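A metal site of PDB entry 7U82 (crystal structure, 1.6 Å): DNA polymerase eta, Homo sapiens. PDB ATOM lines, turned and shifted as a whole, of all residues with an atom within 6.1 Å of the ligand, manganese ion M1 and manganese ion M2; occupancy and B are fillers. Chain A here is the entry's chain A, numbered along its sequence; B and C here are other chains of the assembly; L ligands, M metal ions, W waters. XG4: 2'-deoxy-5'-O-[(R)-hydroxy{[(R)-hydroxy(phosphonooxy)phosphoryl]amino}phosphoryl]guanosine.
O2A of the ligand lies close to O3' of DT 8 of chain C, 2.7 Å away.
O2B of the ligand sits at hydrogen-bond distance from N of Phe 20, at 3.3 Å.
The side-chain amide oxygen (OE1) of Gln 41 lies within hydrogen-bond range of a nitrogen (N2) of the ligand (3.3 Å).
An oxygen (O3G) of the ligand sits at hydrogen-bond distance from the side-chain hydroxyl of Tyr 55, at 2.6 Å.
N3 of DA 5 of chain B is in hydrogen-bond range of N1 of the ligand.
The side-chain amino group of Lys 234 lies within salt-bridge range of an oxygen (O3G) of the ligand, at 3.0 Å.
O4' of DA 5 of chain B lies within hydrogen-bond range of N2 of the ligand, at 3.2 Å.
N of Phe 21 sits at hydrogen-bond distance from O3' of the ligand (3.0 Å).
A nitrogen (N1) of the ligand lies within hydrogen-bond range of O2 of DT 4 of chain B (2.6 Å).
The guanidinium group (NH2) of Arg 64 is in hydrogen-bond range of an oxygen (O6) of the ligand (3.1 Å).
NH2 of Arg 58 is in salt-bridge range of O1G of the ligand, at 3.2 Å.
O3G of the ligand sits at hydrogen-bond distance from N of Cys 19 (2.8 Å).
The side-chain carboxylate (OE2) of Glu 119 is in salt-bridge range of the side-chain amino group (NZ) of Lys 227 (2.7 Å).
The backbone carbonyl oxygen (O) of Asp 16 sits at hydrogen-bond distance from the side-chain amino group (NZ) of Lys 234 (3.2 Å).
NZ of Lys 227 lies close to OD2 of Asp 16 (3.7 Å).
The backbone NH (N) of Asp 118 lies within hydrogen-bond range of the side-chain hydroxyl (OG) of Ser 116.
The side-chain amino group of Lys 234 lies close to the backbone carbonyl oxygen of Met 17 (3.4 Å).
O2 of DT 4 of chain B lies within hydrogen-bond range of NE2 of Gln 41 (3.1 Å).
O4 of DT 3 of chain B sits at hydrogen-bond distance from NH2 of Arg 64 (2.7 Å).
OG of Ser 116 is in hydrogen-bond range of N of Glu 119, 3.3 Å away.
Merely in contact with the ligand: Asp 18 (3.3 Å), Ile 51 (3.5 Å), Ala 52 (3.5 Å), Leu 92 (3.95 Å), Ile 117 (3.9 Å) and DT 3 of chain B (3.8 Å).
Hydrophobic or aromatic side chains that line the ligand: Phe 20, Phe 21, Ile 51, Ala 52, Tyr 55, Leu 92 and Ile 117.
Residues that only touch manganese ion M1: Ser 116 (3.8 Å).
Of the 26 residues printed, 4 come within 4 Å of manganese ion M1.
The nearest printed residue that does not touch manganese ion M1 is Lys 227 (4.2 Å).
Lys 234 touches manganese ion M2 (NZ to MN, 3.9 Å).
Manganese ion M1 is bound by OD1 of Asp 118 (2.0 Å), water W2 (2.1 Å), OD2 of Asp 16 (2.2 Å), OE1 of Glu 119 (2.2 Å), O1A of the ligand (2.3 Å) and water W4 (2.3 Å).
Manganese ion M2 is bound by the side-chain carboxylate (OD1) of Asp 16, the backbone carbonyl oxygen (O) of Met 17, the side-chain carboxylate (OD2) of Asp 118, an oxygen (O2G) of the ligand, an oxygen (O1B) of the ligand and an oxygen (O1A) of the ligand.
Manganese ion M2 has six donor atoms within binding distance.
Water W2 bridges an oxygen (O5') of the ligand (3.3 Å) and the side-chain hydroxyl (OG) of Ser 116 (3.3 Å).
Water W4 lies within hydrogen-bond range of NZ of Lys 227 (2.9 Å) and O2A of the ligand (3.2 Å).
Water W6 lies within hydrogen-bond range of an oxygen (O2B) of the ligand (2.7 Å), the backbone NH of Val 53 (2.8 Å) and the guanidinium group of Arg 58 (2.9 Å).
Water W5 lies within hydrogen-bond range of N3A of the ligand (3.0 Å) and O of Ile 51 (3.1 Å).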
ATOM      1  N   ASP A  16     -15.871  -7.116  30.706  1.00  0.00           N
ATOM      2  CA  ASP A  16     -15.051  -6.945  29.496  1.00  0.00           C
ATOM      3  C   ASP A  16     -13.577  -6.820  29.885  1.00  0.00           C
ATOM      4  O   ASP A  16     -13.248  -5.947  30.680  1.00  0.00           O
ATOM      5  CB  ASP A  16     -15.456  -5.705  28.734  1.00  0.00           C
ATOM      6  CG  ASP A  16     -14.710  -5.568  27.439  1.00  0.00           C
ATOM      7  OD1 ASP A  16     -13.619  -5.029  27.458  1.00  0.00           O
ATOM      8  OD2 ASP A  16     -15.270  -5.983  26.419  1.00  0.00           O
ATOM      9  N   MET A  17     -12.756  -7.664  29.281  1.00  0.00           N
ATOM     10  CA  MET A  17     -11.322  -7.658  29.648  1.00  0.00           C
ATOM     11  C   MET A  17     -10.668  -6.349  29.201  1.00  0.00           C
ATOM     12  O   MET A  17     -10.939  -5.875  28.113  1.00  0.00           O
ATOM     13  CB  MET A  17     -10.603  -8.855  29.038  1.00  0.00           C
ATOM     14  CG  MET A  17     -11.275 -10.182  29.315  1.00  0.00           C
ATOM     15  SD  MET A  17     -11.528 -10.470  31.071  1.00  0.00           S
ATOM     16  CE  MET A  17      -9.846 -10.488  31.645  1.00  0.00           C
ATOM     17  N   ASP A  18      -9.833  -5.785  30.055  1.00  0.00           N
ATOM     18  CA  ASP A  18      -9.108  -4.553  29.681  1.00  0.00           C
ATOM     19  C   ASP A  18      -8.025  -4.870  28.661  1.00  0.00           C
ATOM     20  O   ASP A  18      -7.303  -5.831  28.864  1.00  0.00           O
ATOM     21  CB  ASP A  18      -8.505  -3.880  30.913  1.00  0.00           C
ATOM     22  CG  ASP A  18      -9.511  -3.480  31.972  1.00  0.00           C
ATOM     23  OD1 ASP A  18     -10.637  -3.135  31.621  1.00  0.00           O
ATOM     24  OD2 ASP A  18      -9.138  -3.512  33.142  1.00  0.00           O
ATOM     25  N   CYS A  19      -7.934  -4.067  27.604  1.00  0.00           N
ATOM     26  CA  CYS A  19      -6.955  -4.236  26.519  1.00  0.00           C
ATOM     27  C   CYS A  19      -6.505  -5.699  26.345  1.00  0.00           C
ATOM     28  O   CYS A  19      -5.314  -6.004  26.497  1.00  0.00           O
ATOM     29  CB  CYS A  19      -5.765  -3.268  26.734  1.00  0.00           C
ATOM     30  SG  CYS A  19      -4.935  -3.245  28.292  1.00  0.00           S
ATOM     31  N   PHE A  20      -7.453  -6.583  26.026  1.00  0.00           N
ATOM     32  CA  PHE A  20      -7.275  -8.021  26.283  1.00  0.00           C
ATOM     33  C   PHE A  20      -6.017  -8.604  25.628  1.00  0.00           C
ATOM     34  O   PHE A  20      -5.203  -9.257  26.300  1.00  0.00           O
ATOM     35  CB  PHE A  20      -8.524  -8.790  25.824  1.00  0.00           C
ATOM     36  CG  PHE A  20      -8.465 -10.267  26.127  1.00  0.00           C
ATOM     37  CD1 PHE A  20      -8.092 -10.705  27.391  1.00  0.00           C
ATOM     38  CD2 PHE A  20      -8.778 -11.207  25.160  1.00  0.00           C
ATOM     39  CE1 PHE A  20      -8.050 -12.073  27.697  1.00  0.00           C
ATOM     40  CE2 PHE A  20      -8.715 -12.554  25.453  1.00  0.00           C
ATOM     41  CZ  PHE A  20      -8.360 -12.984  26.716  1.00  0.00           C
ATOM     42  N   PHE A  21      -5.847  -8.433  24.306  1.00  0.00           N
ATOM     43  CA  PHE A  21      -4.689  -9.087  23.693  1.00  0.00           C
ATOM     44  C   PHE A  21      -3.380  -8.559  24.271  1.00  0.00           C
ATOM     45  O   PHE A  21      -2.390  -9.303  24.370  1.00  0.00           O
ATOM     46  CB  PHE A  21      -4.653  -8.932  22.160  1.00  0.00           C
ATOM     47  CG  PHE A  21      -5.711  -9.713  21.400  1.00  0.00           C
ATOM     48  CD1 PHE A  21      -6.836 -10.251  22.008  1.00  0.00           C
ATOM     49  CD2 PHE A  21      -5.539  -9.895  20.022  1.00  0.00           C
ATOM     50  CE1 PHE A  21      -7.799 -10.944  21.234  1.00  0.00           C
ATOM     51  CE2 PHE A  21      -6.475 -10.599  19.260  1.00  0.00           C
ATOM     52  CZ  PHE A  21      -7.601 -11.115  19.864  1.00  0.00           C
ATOM     53  N   VAL A  22      -3.344  -7.254  24.633  1.00  0.00           N
ATOM     54  CA  VAL A  22      -2.169  -6.720  25.291  1.00  0.00           C
ATOM     55  C   VAL A  22      -1.931  -7.430  26.618  1.00  0.00           C
ATOM     56  O   VAL A  22      -0.803  -7.828  26.916  1.00  0.00           O
ATOM     57  CB  VAL A  22      -2.309  -5.195  25.486  1.00  0.00           C
ATOM     58  CG1 VAL A  22      -1.292  -4.688  26.502  1.00  0.00           C
ATOM     59  CG2 VAL A  22      -2.125  -4.501  24.143  1.00  0.00           C
ATOM     60  N   GLN A  41      -1.040  -6.924  13.968  1.00  0.00           N
ATOM     61  CA  GLN A  41      -1.005  -8.058  13.053  1.00  0.00           C
ATOM     62  C   GLN A  41      -0.184  -7.691  11.823  1.00  0.00           C
ATOM     63  O   GLN A  41      -0.380  -6.617  11.239  1.00  0.00           O
ATOM     64  CB  GLN A  41      -2.394  -8.588  12.657  1.00  0.00           C
ATOM     65  CG  GLN A  41      -3.489  -8.419  13.691  1.00  0.00           C
ATOM     66  CD  GLN A  41      -4.858  -8.917  13.199  1.00  0.00           C
ATOM     67  OE1 GLN A  41      -5.238 -10.058  13.458  1.00  0.00           O
ATOM     68  NE2 GLN A  41      -5.587  -8.052  12.505  1.00  0.00           N
ATOM     69  N   ILE A  51      -4.360  -3.707  16.836  1.00  0.00           N
ATOM     70  CA  ILE A  51      -5.696  -4.164  17.208  1.00  0.00           C
ATOM     71  C   ILE A  51      -5.972  -4.050  18.698  1.00  0.00           C
ATOM     72  O   ILE A  51      -7.127  -4.219  19.096  1.00  0.00           O
ATOM     73  CB  ILE A  51      -5.959  -5.606  16.725  1.00  0.00           C
ATOM     74  CG1 ILE A  51      -4.881  -6.582  17.225  1.00  0.00           C
ATOM     75  CG2 ILE A  51      -6.161  -5.639  15.212  1.00  0.00           C
ATOM     76  CD1 ILE A  51      -5.218  -8.055  16.970  1.00  0.00           C
ATOM     77  N   ALA A  52      -4.975  -3.717  19.539  1.00  0.00           N
ATOM     78  CA  ALA A  52      -5.184  -3.610  20.969  1.00  0.00           C
ATOM     79  C   ALA A  52      -4.096  -2.715  21.550  1.00  0.00           C
ATOM     80  O   ALA A  52      -2.959  -2.770  21.085  1.00  0.00           O
ATOM     81  CB  ALA A  52      -5.150  -4.981  21.660  1.00  0.00           C
ATOM     82  N   VAL A  53      -4.453  -1.897  22.554  1.00  0.00           N
ATOM     83  CA  VAL A  53      -3.584  -0.819  23.035  1.00  0.00           C
ATOM     84  C   VAL A  53      -3.667  -0.710  24.556  1.00  0.00           C
ATOM     85  O   VAL A  53      -4.759  -0.562  25.107  1.00  0.00           O
ATOM     86  CB  VAL A  53      -3.957   0.537  22.396  1.00  0.00           C
ATOM     87  CG1 VAL A  53      -2.971   1.593  22.789  1.00  0.00           C
ATOM     88  CG2 VAL A  53      -3.990   0.419  20.906  1.00  0.00           C
ATOM     89  N   TYR A  55      -3.432   0.992  28.257  1.00  0.00           N
ATOM     90  CA  TYR A  55      -3.930   2.311  28.656  1.00  0.00           C
ATOM     91  C   TYR A  55      -2.800   3.341  28.730  1.00  0.00           C
ATOM     92  O   TYR A  55      -3.018   4.533  28.421  1.00  0.00           O
ATOM     93  CB  TYR A  55      -4.688   2.172  29.972  1.00  0.00           C
ATOM     94  CG  TYR A  55      -6.067   1.608  29.673  1.00  0.00           C
ATOM     95  CD1 TYR A  55      -6.252   0.257  29.429  1.00  0.00           C
ATOM     96  CD2 TYR A  55      -7.164   2.455  29.567  1.00  0.00           C
ATOM     97  CE1 TYR A  55      -7.511  -0.262  29.123  1.00  0.00           C
ATOM     98  CE2 TYR A  55      -8.420   1.968  29.266  1.00  0.00           C
ATOM     99  CZ  TYR A  55      -8.587   0.609  29.024  1.00  0.00           C
ATOM    100  OH  TYR A  55      -9.853   0.126  28.722  1.00  0.00           O
ATOM    101  N   ARG A  58      -2.500   4.440  25.207  1.00  0.00           N
ATOM    102  CA  ARG A  58      -3.646   5.255  24.824  1.00  0.00           C
ATOM    103  C   ARG A  58      -3.451   6.705  25.234  1.00  0.00           C
ATOM    104  O   ARG A  58      -3.944   7.609  24.544  1.00  0.00           O
ATOM    105  CB  ARG A  58      -4.932   4.729  25.460  1.00  0.00           C
ATOM    106  CG  ARG A  58      -5.287   3.338  25.040  1.00  0.00           C
ATOM    107  CD  ARG A  58      -6.620   2.946  25.625  1.00  0.00           C
ATOM    108  NE  ARG A  58      -6.847   1.528  25.401  1.00  0.00           N
ATOM    109  CZ  ARG A  58      -8.011   0.925  25.544  1.00  0.00           C
ATOM    110  NH1 ARG A  58      -9.090   1.597  25.932  1.00  0.00           N
ATOM    111  NH2 ARG A  58      -8.105  -0.374  25.262  1.00  0.00           N
ATOM    112  N   ARG A  64      -6.596   1.440  18.310  1.00  0.00           N
ATOM    113  CA  ARG A  64      -6.819   0.381  17.342  1.00  0.00           C
ATOM    114  C   ARG A  64      -7.071   1.001  15.968  1.00  0.00           C
ATOM    115  O   ARG A  64      -7.496   2.153  15.857  1.00  0.00           O
ATOM    116  CB  ARG A  64      -7.987  -0.529  17.786  1.00  0.00           C
ATOM    117  CG  ARG A  64      -9.376  -0.123  17.344  1.00  0.00           C
ATOM    118  CD  ARG A  64     -10.438  -1.222  17.595  1.00  0.00           C
ATOM    119  NE  ARG A  64     -10.669  -2.124  16.471  1.00  0.00           N
ATOM    120  CZ  ARG A  64     -11.408  -1.810  15.418  1.00  0.00           C
ATOM    121  NH1 ARG A  64     -11.965  -0.612  15.289  1.00  0.00           N
ATOM    122  NH2 ARG A  64     -11.597  -2.718  14.446  1.00  0.00           N
ATOM    123  N   LEU A  92      -4.980 -16.525  15.831  1.00  0.00           N
ATOM    124  CA  LEU A  92      -5.393 -15.939  17.105  1.00  0.00           C
ATOM    125  C   LEU A  92      -5.613 -16.976  18.208  1.00  0.00           C
ATOM    126  O   LEU A  92      -6.279 -16.685  19.204  1.00  0.00           O
ATOM    127  CB  LEU A  92      -6.648 -15.091  16.908  1.00  0.00           C
ATOM    128  CG  LEU A  92      -6.553 -14.068  15.776  1.00  0.00           C
ATOM    129  CD1 LEU A  92      -7.843 -13.328  15.565  1.00  0.00           C
ATOM    130  CD2 LEU A  92      -5.382 -13.138  16.037  1.00  0.00           C
ATOM    131  N   SER A 116     -18.174 -11.850  22.961  1.00  0.00           N
ATOM    132  CA  SER A 116     -17.030 -11.685  22.077  1.00  0.00           C
ATOM    133  C   SER A 116     -15.892 -12.484  22.681  1.00  0.00           C
ATOM    134  O   SER A 116     -16.053 -13.126  23.713  1.00  0.00           O
ATOM    135  CB  SER A 116     -16.627 -10.223  21.960  1.00  0.00           C
ATOM    136  OG  SER A 116     -15.816  -9.917  23.078  1.00  0.00           O
ATOM    137  N   ILE A 117     -14.715 -12.430  22.038  1.00  0.00           N
ATOM    138  CA  ILE A 117     -13.540 -13.074  22.608  1.00  0.00           C
ATOM    139  C   ILE A 117     -13.202 -12.556  23.995  1.00  0.00           C
ATOM    140  O   ILE A 117     -12.538 -13.258  24.765  1.00  0.00           O
ATOM    141  CB  ILE A 117     -12.348 -12.889  21.640  1.00  0.00           C
ATOM    142  CG1 ILE A 117     -11.243 -13.881  21.971  1.00  0.00           C
ATOM    143  CG2 ILE A 117     -11.849 -11.455  21.689  1.00  0.00           C
ATOM    144  CD1 ILE A 117     -10.237 -13.970  20.843  1.00  0.00           C
ATOM    145  N   ASP A 118     -13.610 -11.341  24.339  1.00  0.00           N
ATOM    146  CA  ASP A 118     -13.146 -10.871  25.644  1.00  0.00           C
ATOM    147  C   ASP A 118     -14.261 -10.348  26.541  1.00  0.00           C
ATOM    148  O   ASP A 118     -13.977  -9.646  27.524  1.00  0.00           O
ATOM    149  CB  ASP A 118     -12.068  -9.795  25.507  1.00  0.00           C
ATOM    150  CG  ASP A 118     -12.611  -8.405  25.450  1.00  0.00           C
ATOM    151  OD1 ASP A 118     -13.667  -8.170  24.813  1.00  0.00           O
ATOM    152  OD2 ASP A 118     -11.986  -7.551  26.127  1.00  0.00           O
ATOM    153  N   GLU A 119     -15.519 -10.687  26.257  1.00  0.00           N
ATOM    154  CA  GLU A 119     -16.534 -10.187  27.148  1.00  0.00           C
ATOM    155  C   GLU A 119     -17.740 -11.105  27.147  1.00  0.00           C
ATOM    156  O   GLU A 119     -18.033 -11.783  26.140  1.00  0.00           O
ATOM    157  CB  GLU A 119     -16.981  -8.779  26.774  1.00  0.00           C
ATOM    158  CG  GLU A 119     -17.907  -8.788  25.588  1.00  0.00           C
ATOM    159  CD  GLU A 119     -17.762  -7.547  24.796  1.00  0.00           C
ATOM    160  OE1 GLU A 119     -16.745  -7.421  24.081  1.00  0.00           O
ATOM    161  OE2 GLU A 119     -18.684  -6.695  24.873  1.00  0.00           O
ATOM    162  N   LYS A 227     -23.501  -2.960  29.346  1.00  0.00           N
ATOM    163  CA  LYS A 227     -22.361  -2.708  28.449  1.00  0.00           C
ATOM    164  C   LYS A 227     -21.912  -1.257  28.536  1.00  0.00           C
ATOM    165  O   LYS A 227     -20.698  -0.947  28.642  1.00  0.00           O
ATOM    166  CB  LYS A 227     -22.772  -3.077  27.018  1.00  0.00           C
ATOM    167  CG  LYS A 227     -21.721  -2.756  25.948  1.00  0.00           C
ATOM    168  CD  LYS A 227     -20.436  -3.586  26.142  1.00  0.00           C
ATOM    169  CE  LYS A 227     -19.402  -3.261  25.041  1.00  0.00           C
ATOM    170  NZ  LYS A 227     -18.103  -4.023  25.143  1.00  0.00           N
ATOM    171  N   LYS A 234     -13.404   2.365  32.755  1.00  0.00           N
ATOM    172  CA  LYS A 234     -12.233   1.517  32.426  1.00  0.00           C
ATOM    173  C   LYS A 234     -10.946   2.330  32.635  1.00  0.00           C
ATOM    174  O   LYS A 234     -10.966   3.530  32.376  1.00  0.00           O
ATOM    175  CB  LYS A 234     -12.336   1.070  30.967  1.00  0.00           C
ATOM    176  CG  LYS A 234     -13.306  -0.057  30.666  1.00  0.00           C
ATOM    177  CD  LYS A 234     -13.024  -0.703  29.331  1.00  0.00           C
ATOM    178  CE  LYS A 234     -13.510  -2.137  29.251  1.00  0.00           C
ATOM    179  NZ  LYS A 234     -12.398  -3.120  29.378  1.00  0.00           N
ATOM    180  N   PRO A 235      -9.817   1.724  33.026  1.00  0.00           N
ATOM    181  CA  PRO A 235      -9.750   0.285  33.303  1.00  0.00           C
ATOM    182  C   PRO A 235      -9.827  -0.197  34.755  1.00  0.00           C
ATOM    183  O   PRO A 235      -9.808   0.607  35.631  1.00  0.00           O
ATOM    184  CB  PRO A 235      -8.325  -0.014  32.827  1.00  0.00           C
ATOM    185  CG  PRO A 235      -7.533   1.199  33.236  1.00  0.00           C
ATOM    186  CD  PRO A 235      -8.505   2.358  33.153  1.00  0.00           C
ATOM    187  P    DT B   3      -6.191   1.568   4.311  1.00  0.00           P
ATOM    188  OP1  DT B   3      -6.803   2.363   3.223  1.00  0.00           O
ATOM    189  OP2  DT B   3      -5.531   2.255   5.450  1.00  0.00           O
ATOM    190  O5'  DT B   3      -7.329   0.592   4.846  1.00  0.00           O
ATOM    191  C5'  DT B   3      -7.430   0.268   6.243  1.00  0.00           C
ATOM    192  C4'  DT B   3      -6.499  -0.867   6.576  1.00  0.00           C
ATOM    193  O4'  DT B   3      -6.372  -0.966   8.019  1.00  0.00           O
ATOM    194  C3'  DT B   3      -6.984  -2.239   6.112  1.00  0.00           C
ATOM    195  O3'  DT B   3      -5.880  -3.089   5.793  1.00  0.00           O
ATOM    196  C2'  DT B   3      -7.681  -2.774   7.338  1.00  0.00           C
ATOM    197  C1'  DT B   3      -6.749  -2.273   8.426  1.00  0.00           C
ATOM    198  N1   DT B   3      -7.415  -2.179   9.725  1.00  0.00           N
ATOM    199  C2   DT B   3      -6.896  -2.891  10.790  1.00  0.00           C
ATOM    200  O2   DT B   3      -5.879  -3.552  10.714  1.00  0.00           O
ATOM    201  N3   DT B   3      -7.617  -2.771  11.954  1.00  0.00           N
ATOM    202  C4   DT B   3      -8.770  -2.051  12.152  1.00  0.00           C
ATOM    203  O4   DT B   3      -9.303  -2.037  13.252  1.00  0.00           O
ATOM    204  C5   DT B   3      -9.262  -1.344  10.987  1.00  0.00           C
ATOM    205  C7   DT B   3     -10.526  -0.544  11.091  1.00  0.00           C
ATOM    206  C6   DT B   3      -8.569  -1.448   9.851  1.00  0.00           C
ATOM    207  P    DT B   4      -6.133  -4.569   5.235  1.00  0.00           P
ATOM    208  OP1  DT B   4      -4.899  -5.012   4.558  1.00  0.00           O
ATOM    209  OP2  DT B   4      -7.428  -4.590   4.537  1.00  0.00           O
ATOM    210  O5'  DT B   4      -6.332  -5.426   6.553  1.00  0.00           O
ATOM    211  C5'  DT B   4      -5.270  -5.677   7.466  1.00  0.00           C
ATOM    212  C4'  DT B   4      -5.661  -6.811   8.372  1.00  0.00           C
ATOM    213  O4'  DT B   4      -6.523  -6.333   9.428  1.00  0.00           O
ATOM    214  C3'  DT B   4      -6.445  -7.927   7.685  1.00  0.00           C
ATOM    215  O3'  DT B   4      -5.904  -9.114   8.257  1.00  0.00           O
ATOM    216  C2'  DT B   4      -7.878  -7.657   8.095  1.00  0.00           C
ATOM    217  C1'  DT B   4      -7.703  -7.109   9.487  1.00  0.00           C
ATOM    218  N1   DT B   4      -8.768  -6.221   9.952  1.00  0.00           N
ATOM    219  C2   DT B   4      -9.048  -6.240  11.291  1.00  0.00           C
ATOM    220  O2   DT B   4      -8.515  -7.014  12.071  1.00  0.00           O
ATOM    221  N3   DT B   4     -10.020  -5.350  11.685  1.00  0.00           N
ATOM    222  C4   DT B   4     -10.658  -4.416  10.909  1.00  0.00           C
ATOM    223  O4   DT B   4     -11.532  -3.712  11.394  1.00  0.00           O
ATOM    224  C5   DT B   4     -10.340  -4.470   9.501  1.00  0.00           C
ATOM    225  C7   DT B   4     -11.046  -3.542   8.564  1.00  0.00           C
ATOM    226  C6   DT B   4      -9.400  -5.335   9.103  1.00  0.00           C
ATOM    227  P    DA B   5      -6.446 -10.530   7.841  1.00  0.00           P
ATOM    228  OP1  DA B   5      -5.290 -11.415   7.659  1.00  0.00           O
ATOM    229  OP2  DA B   5      -7.406 -10.374   6.761  1.00  0.00           O
ATOM    230  O5'  DA B   5      -7.258 -10.993   9.126  1.00  0.00           O
ATOM    231  C5'  DA B   5      -6.612 -11.111  10.391  1.00  0.00           C
ATOM    232  C4'  DA B   5      -7.578 -11.644  11.414  1.00  0.00           C
ATOM    233  O4'  DA B   5      -8.525 -10.607  11.755  1.00  0.00           O
ATOM    234  C3'  DA B   5      -8.402 -12.841  10.942  1.00  0.00           C
ATOM    235  O3'  DA B   5      -8.561 -13.741  12.035  1.00  0.00           O
ATOM    236  C2'  DA B   5      -9.721 -12.198  10.524  1.00  0.00           C
ATOM    237  C1'  DA B   5      -9.845 -11.076  11.532  1.00  0.00           C
ATOM    238  N9   DA B   5     -10.651  -9.950  11.070  1.00  0.00           N
ATOM    239  C8   DA B   5     -10.758  -9.457   9.798  1.00  0.00           C
ATOM    240  N7   DA B   5     -11.541  -8.418   9.704  1.00  0.00           N
ATOM    241  C5   DA B   5     -11.974  -8.196  11.004  1.00  0.00           C
ATOM    242  C6   DA B   5     -12.818  -7.238  11.570  1.00  0.00           C
ATOM    243  N6   DA B   5     -13.431  -6.282  10.872  1.00  0.00           N
ATOM    244  N1   DA B   5     -13.043  -7.305  12.906  1.00  0.00           N
ATOM    245  C2   DA B   5     -12.435  -8.269  13.606  1.00  0.00           C
ATOM    246  N3   DA B   5     -11.622  -9.226  13.181  1.00  0.00           N
ATOM    247  C4   DA B   5     -11.421  -9.134  11.861  1.00  0.00           C
ATOM    248  P    DT C   8     -18.137  -1.752  19.765  1.00  0.00           P
ATOM    249  OP1  DT C   8     -18.393  -1.797  21.219  1.00  0.00           O
ATOM    250  OP2  DT C   8     -18.275  -0.475  19.018  1.00  0.00           O
ATOM    251  O5'  DT C   8     -16.669  -2.313  19.513  1.00  0.00           O
ATOM    252  C5'  DT C   8     -16.314  -3.663  19.847  1.00  0.00           C
ATOM    253  C4'  DT C   8     -14.969  -3.990  19.244  1.00  0.00           C
ATOM    254  O4'  DT C   8     -15.134  -4.461  17.880  1.00  0.00           O
ATOM    255  C3'  DT C   8     -14.003  -2.810  19.162  1.00  0.00           C
ATOM    256  O3'  DT C   8     -12.674  -3.197  19.479  1.00  0.00           O
ATOM    257  C2'  DT C   8     -14.012  -2.447  17.698  1.00  0.00           C
ATOM    258  C1'  DT C   8     -14.107  -3.846  17.128  1.00  0.00           C
ATOM    259  N1   DT C   8     -14.460  -3.906  15.719  1.00  0.00           N
ATOM    260  C2   DT C   8     -14.146  -5.043  15.028  1.00  0.00           C
ATOM    261  O2   DT C   8     -13.681  -6.034  15.570  1.00  0.00           O
ATOM    262  N3   DT C   8     -14.426  -5.003  13.685  1.00  0.00           N
ATOM    263  C4   DT C   8     -14.949  -3.945  12.981  1.00  0.00           C
ATOM    264  O4   DT C   8     -15.141  -4.057  11.773  1.00  0.00           O
ATOM    265  C5   DT C   8     -15.224  -2.757  13.755  1.00  0.00           C
ATOM    266  C7   DT C   8     -15.797  -1.561  13.070  1.00  0.00           C
ATOM    267  C6   DT C   8     -14.962  -2.793  15.068  1.00  0.00           C
HETATM  268  N1  XG4 L   1      -9.375  -7.499  14.494  1.00  0.00           N
HETATM  269  C2  XG4 L   1      -8.896  -8.461  15.335  1.00  0.00           C
HETATM  270  N2  XG4 L   1      -8.265  -9.481  14.757  1.00  0.00           N
HETATM  271  N3  XG4 L   1      -8.963  -8.445  16.668  1.00  0.00           N
HETATM  272  C4  XG4 L   1      -9.575  -7.371  17.156  1.00  0.00           C
HETATM  273  C5  XG4 L   1     -10.091  -6.349  16.448  1.00  0.00           C
HETATM  274  C6  XG4 L   1      -9.969  -6.424  15.042  1.00  0.00           C
HETATM  275  O6  XG4 L   1     -10.378  -5.511  14.301  1.00  0.00           O
HETATM  276  N7  XG4 L   1     -10.661  -5.394  17.288  1.00  0.00           N
HETATM  277  C8  XG4 L   1     -10.470  -5.880  18.499  1.00  0.00           C
HETATM  278  N9  XG4 L   1      -9.805  -7.081  18.487  1.00  0.00           N
HETATM  279  PA  XG4 L   1     -12.139  -4.920  22.930  1.00  0.00           P
HETATM  280  PB  XG4 L   1      -9.714  -4.197  24.441  1.00  0.00           P
HETATM  281  PG  XG4 L   1     -10.778  -2.265  26.271  1.00  0.00           P
HETATM  282  C1' XG4 L   1      -9.336  -7.893  19.617  1.00  0.00           C
HETATM  283  O1A XG4 L   1     -12.837  -5.332  24.157  1.00  0.00           O
HETATM  284  O1B XG4 L   1     -10.051  -5.369  25.262  1.00  0.00           O
HETATM  285  O1G XG4 L   1     -11.174  -0.891  25.751  1.00  0.00           O
HETATM  286  C2' XG4 L   1      -8.183  -7.264  20.392  1.00  0.00           C
HETATM  287  O2A XG4 L   1     -13.031  -4.018  21.996  1.00  0.00           O
HETATM  288  O2B XG4 L   1      -8.328  -4.344  23.759  1.00  0.00           O
HETATM  289  O2G XG4 L   1     -11.922  -3.264  26.284  1.00  0.00           O
HETATM  290  C3' XG4 L   1      -8.838  -6.779  21.671  1.00  0.00           C
HETATM  291  O3' XG4 L   1      -7.881  -6.848  22.726  1.00  0.00           O
HETATM  292  N3A XG4 L   1     -10.792  -4.031  23.228  1.00  0.00           N
HETATM  293  O3B XG4 L   1      -9.700  -2.866  25.265  1.00  0.00           O
HETATM  294  O3G XG4 L   1     -10.084  -2.237  27.615  1.00  0.00           O
HETATM  295  C4' XG4 L   1      -9.963  -7.780  21.866  1.00  0.00           C
HETATM  296  O4' XG4 L   1     -10.422  -8.068  20.533  1.00  0.00           O
HETATM  297  C5' XG4 L   1     -11.125  -7.321  22.712  1.00  0.00           C
HETATM  298  O5' XG4 L   1     -11.718  -6.168  22.054  1.00  0.00           O
HETATM  299 MN    MN M   1     -14.751  -6.506  24.367  1.00  0.00          MN
HETATM  300 MN    MN M   2     -11.950  -5.432  26.310  1.00  0.00          MN
HETATM  301  O   HOH W   1     -11.089   0.015  23.280  1.00  0.00           O
HETATM  302  O   HOH W   2     -14.920  -6.855  22.275  1.00  0.00           O
HETATM  303  O   HOH W   3     -14.526  -2.493  25.650  1.00  0.00           O
HETATM  304  O   HOH W   4     -15.558  -4.420  23.875  1.00  0.00           O
HETATM  305  O   HOH W   5      -9.403  -3.050  20.759  1.00  0.00           O
HETATM  306  O   HOH W   6      -7.155  -2.000  23.070  1.00  0.00           O
